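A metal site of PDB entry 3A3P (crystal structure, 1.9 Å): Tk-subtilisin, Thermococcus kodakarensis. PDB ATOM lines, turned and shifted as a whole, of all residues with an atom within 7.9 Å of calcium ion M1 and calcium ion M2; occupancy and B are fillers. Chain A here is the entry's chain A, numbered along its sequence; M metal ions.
OD2 of Asp 153 sits close to N of Asp 155 (2.8 Å).
OD1 of Asp 143 sits close to N of Gly 146, at 3.2 Å.
The side-chain carboxylate of Asp 143 sits at hydrogen-bond distance from the backbone NH of Gly 148, 2.7 Å away.
N of Lys 144 is in hydrogen-bond range of OD1 of Asp 156, at 2.7 Å.
Within 4 Å of calcium ion M1: Asp 143, Asp 145, Asp 147, Ile 149, Asp 153 and Asp 156.
The nearest printed residue that does not touch calcium ion M1 is Ile 150 (4.6 Å).
Within 4 Å of calcium ion M2: Asp 145, Asp 147 and Asp 153.
The nearest printed residue that does not touch calcium ion M2 is Asp 155 (4.1 Å).
Calcium ion M1 is bound by OD1 of Asp 143 (2.2 Å), OD2 of Asp 156 (2.3 Å), O of Ile 149 (2.3 Å), OD1 of Asp 153 (2.4 Å), OD2 of Asp 145 (2.4 Å) and OD1 of Asp 147 (2.4 Å).
Calcium ion M2 is bound by the side-chain carboxylate (OD2) of Asp 147 (1.8 Å), the side-chain carboxylate (OD1) of Asp 153 (2.0 Å), the side-chain carboxylate (OD1) of Asp 145 (2.0 Å) and the side-chain carboxylate (OD2) of Asp 153 (2.9 Å).
Slightly farther from calcium ion M2 lies OD2 of Asp 145 (3.1 Å).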
ATOM      1  N   ALA A 142      18.648 -28.779  12.023  1.00  0.00           N
ATOM      2  CA  ALA A 142      18.558 -27.349  11.703  1.00  0.00           C
ATOM      3  C   ALA A 142      17.091 -26.890  11.652  1.00  0.00           C
ATOM      4  O   ALA A 142      16.730 -25.901  12.308  1.00  0.00           O
ATOM      5  CB  ALA A 142      19.253 -27.032  10.363  1.00  0.00           C
ATOM      6  N   ASP A 143      16.258 -27.613  10.874  1.00  0.00           N
ATOM      7  CA  ASP A 143      14.886 -27.193  10.573  1.00  0.00           C
ATOM      8  C   ASP A 143      13.976 -28.385  10.768  1.00  0.00           C
ATOM      9  O   ASP A 143      13.665 -29.107   9.832  1.00  0.00           O
ATOM     10  CB  ASP A 143      14.821 -26.635   9.134  1.00  0.00           C
ATOM     11  CG  ASP A 143      13.407 -26.162   8.694  1.00  0.00           C
ATOM     12  OD1 ASP A 143      12.502 -25.909   9.531  1.00  0.00           O
ATOM     13  OD2 ASP A 143      13.204 -26.014   7.457  1.00  0.00           O
ATOM     14  N   LYS A 144      13.533 -28.601  11.994  1.00  0.00           N
ATOM     15  CA  LYS A 144      12.838 -29.847  12.319  1.00  0.00           C
ATOM     16  C   LYS A 144      11.462 -30.006  11.638  1.00  0.00           C
ATOM     17  O   LYS A 144      11.073 -31.112  11.283  1.00  0.00           O
ATOM     18  CB  LYS A 144      12.847 -30.025  13.834  1.00  0.00           C
ATOM     19  CG  LYS A 144      11.554 -30.371  14.547  1.00  0.00           C
ATOM     20  CD  LYS A 144      11.864 -30.455  16.058  1.00  0.00           C
ATOM     21  CE  LYS A 144      13.204 -31.213  16.341  1.00  0.00           C
ATOM     22  NZ  LYS A 144      13.190 -32.739  16.523  1.00  0.00           N
ATOM     23  N   ASP A 145      10.758 -28.896  11.404  1.00  0.00           N
ATOM     24  CA  ASP A 145       9.460 -28.969  10.742  1.00  0.00           C
ATOM     25  C   ASP A 145       9.551 -28.645   9.264  1.00  0.00           C
ATOM     26  O   ASP A 145       8.538 -28.486   8.607  1.00  0.00           O
ATOM     27  CB  ASP A 145       8.437 -28.072  11.417  1.00  0.00           C
ATOM     28  CG  ASP A 145       8.882 -26.632  11.522  1.00  0.00           C
ATOM     29  OD1 ASP A 145       8.151 -25.833  12.145  1.00  0.00           O
ATOM     30  OD2 ASP A 145       9.955 -26.285  10.997  1.00  0.00           O
ATOM     31  N   GLY A 146      10.764 -28.492   8.752  1.00  0.00           N
ATOM     32  CA  GLY A 146      10.952 -28.371   7.289  1.00  0.00           C
ATOM     33  C   GLY A 146      10.312 -27.195   6.569  1.00  0.00           C
ATOM     34  O   GLY A 146      10.086 -27.257   5.343  1.00  0.00           O
ATOM     35  N   ASP A 147      10.057 -26.083   7.284  1.00  0.00           N
ATOM     36  CA  ASP A 147       9.395 -24.930   6.680  1.00  0.00           C
ATOM     37  C   ASP A 147      10.380 -23.864   6.208  1.00  0.00           C
ATOM     38  O   ASP A 147       9.978 -22.809   5.732  1.00  0.00           O
ATOM     39  CB  ASP A 147       8.356 -24.313   7.648  1.00  0.00           C
ATOM     40  CG  ASP A 147       8.938 -24.001   9.034  1.00  0.00           C
ATOM     41  OD1 ASP A 147      10.188 -23.905   9.157  1.00  0.00           O
ATOM     42  OD2 ASP A 147       8.149 -23.866  10.019  1.00  0.00           O
ATOM     43  N   GLY A 148      11.680 -24.142   6.296  1.00  0.00           N
ATOM     44  CA  GLY A 148      12.683 -23.168   5.835  1.00  0.00           C
ATOM     45  C   GLY A 148      12.925 -22.033   6.821  1.00  0.00           C
ATOM     46  O   GLY A 148      13.696 -21.117   6.517  1.00  0.00           O
ATOM     47  N   ILE A 149      12.258 -22.055   7.977  1.00  0.00           N
ATOM     48  CA  ILE A 149      12.481 -21.019   8.990  1.00  0.00           C
ATOM     49  C   ILE A 149      13.328 -21.650  10.085  1.00  0.00           C
ATOM     50  O   ILE A 149      12.981 -22.675  10.633  1.00  0.00           O
ATOM     51  CB  ILE A 149      11.166 -20.477   9.561  1.00  0.00           C
ATOM     52  CG1 ILE A 149      10.197 -20.167   8.414  1.00  0.00           C
ATOM     53  CG2 ILE A 149      11.411 -19.267  10.489  1.00  0.00           C
ATOM     54  CD1 ILE A 149       8.884 -19.743   8.867  1.00  0.00           C
ATOM     55  N   ILE A 150      14.453 -21.026  10.406  1.00  0.00           N
ATOM     56  CA  ILE A 150      15.363 -21.608  11.382  1.00  0.00           C
ATOM     57  C   ILE A 150      15.502 -20.673  12.585  1.00  0.00           C
ATOM     58  O   ILE A 150      14.838 -20.917  13.612  1.00  0.00           O
ATOM     59  CB  ILE A 150      16.693 -22.058  10.717  1.00  0.00           C
ATOM     60  CG1 ILE A 150      16.405 -23.123   9.617  1.00  0.00           C
ATOM     61  CG2 ILE A 150      17.700 -22.615  11.805  1.00  0.00           C
ATOM     62  CD1 ILE A 150      17.566 -23.471   8.726  1.00  0.00           C
ATOM     63  N   ALA A 151      16.350 -19.627  12.490  1.00  0.00           N
ATOM     64  CA  ALA A 151      16.335 -18.542  13.489  1.00  0.00           C
ATOM     65  C   ALA A 151      14.925 -17.979  13.602  1.00  0.00           C
ATOM     66  O   ALA A 151      14.256 -17.688  12.617  1.00  0.00           O
ATOM     67  CB  ALA A 151      17.311 -17.406  13.102  1.00  0.00           C
ATOM     68  N   GLY A 152      14.458 -17.826  14.839  1.00  0.00           N
ATOM     69  CA  GLY A 152      13.138 -17.249  15.067  1.00  0.00           C
ATOM     70  C   GLY A 152      11.944 -18.197  14.978  1.00  0.00           C
ATOM     71  O   GLY A 152      10.827 -17.753  15.244  1.00  0.00           O
ATOM     72  N   ASP A 153      12.166 -19.457  14.573  1.00  0.00           N
ATOM     73  CA  ASP A 153      11.091 -20.461  14.530  1.00  0.00           C
ATOM     74  C   ASP A 153      10.952 -21.067  15.916  1.00  0.00           C
ATOM     75  O   ASP A 153      11.887 -21.725  16.389  1.00  0.00           O
ATOM     76  CB  ASP A 153      11.376 -21.559  13.498  1.00  0.00           C
ATOM     77  CG  ASP A 153      10.174 -22.503  13.313  1.00  0.00           C
ATOM     78  OD1 ASP A 153      10.074 -23.180  12.281  1.00  0.00           O
ATOM     79  OD2 ASP A 153       9.344 -22.598  14.232  1.00  0.00           O
ATOM     80  N   PRO A 154       9.808 -20.848  16.584  1.00  0.00           N
ATOM     81  CA  PRO A 154       9.712 -21.394  17.943  1.00  0.00           C
ATOM     82  C   PRO A 154       9.680 -22.905  17.987  1.00  0.00           C
ATOM     83  O   PRO A 154       9.841 -23.486  19.052  1.00  0.00           O
ATOM     84  CB  PRO A 154       8.405 -20.800  18.478  1.00  0.00           C
ATOM     85  CG  PRO A 154       7.593 -20.477  17.221  1.00  0.00           C
ATOM     86  CD  PRO A 154       8.621 -20.042  16.215  1.00  0.00           C
ATOM     87  N   ASP A 155       9.493 -23.559  16.853  1.00  0.00           N
ATOM     88  CA  ASP A 155       9.572 -25.019  16.796  1.00  0.00           C
ATOM     89  C   ASP A 155      11.006 -25.538  16.802  1.00  0.00           C
ATOM     90  O   ASP A 155      11.242 -26.674  17.218  1.00  0.00           O
ATOM     91  CB  ASP A 155       8.824 -25.576  15.579  1.00  0.00           C
ATOM     92  CG  ASP A 155       8.664 -27.089  15.622  1.00  0.00           C
ATOM     93  OD1 ASP A 155       9.160 -27.779  14.686  1.00  0.00           O
ATOM     94  OD2 ASP A 155       8.072 -27.584  16.614  1.00  0.00           O
ATOM     95  N   ASP A 156      11.972 -24.711  16.369  1.00  0.00           N
ATOM     96  CA  ASP A 156      13.372 -25.089  16.299  1.00  0.00           C
ATOM     97  C   ASP A 156      14.130 -24.463  17.455  1.00  0.00           C
ATOM     98  O   ASP A 156      13.553 -23.682  18.214  1.00  0.00           O
ATOM     99  CB  ASP A 156      13.972 -24.657  14.970  1.00  0.00           C
ATOM    100  CG  ASP A 156      13.535 -25.546  13.831  1.00  0.00           C
ATOM    101  OD1 ASP A 156      13.840 -26.759  13.895  1.00  0.00           O
ATOM    102  OD2 ASP A 156      12.890 -25.039  12.889  1.00  0.00           O
ATOM    103  N   ASP A 157      15.430 -24.764  17.552  1.00  0.00           N
ATOM    104  CA  ASP A 157      16.248 -24.285  18.659  1.00  0.00           C
ATOM    105  C   ASP A 157      17.546 -23.622  18.229  1.00  0.00           C
ATOM    106  O   ASP A 157      18.535 -23.608  18.981  1.00  0.00           O
ATOM    107  CB  ASP A 157      16.547 -25.438  19.608  1.00  0.00           C
ATOM    108  CG  ASP A 157      17.258 -26.585  18.924  1.00  0.00           C
ATOM    109  OD1 ASP A 157      17.456 -27.615  19.618  1.00  0.00           O
ATOM    110  OD2 ASP A 157      17.604 -26.508  17.689  1.00  0.00           O
HETATM  111 CA    CA M   1      11.599 -24.529  11.032  1.00  0.00          CA
HETATM  112 CA    CA M   2       8.258 -23.853  11.860  1.00  0.00          CA
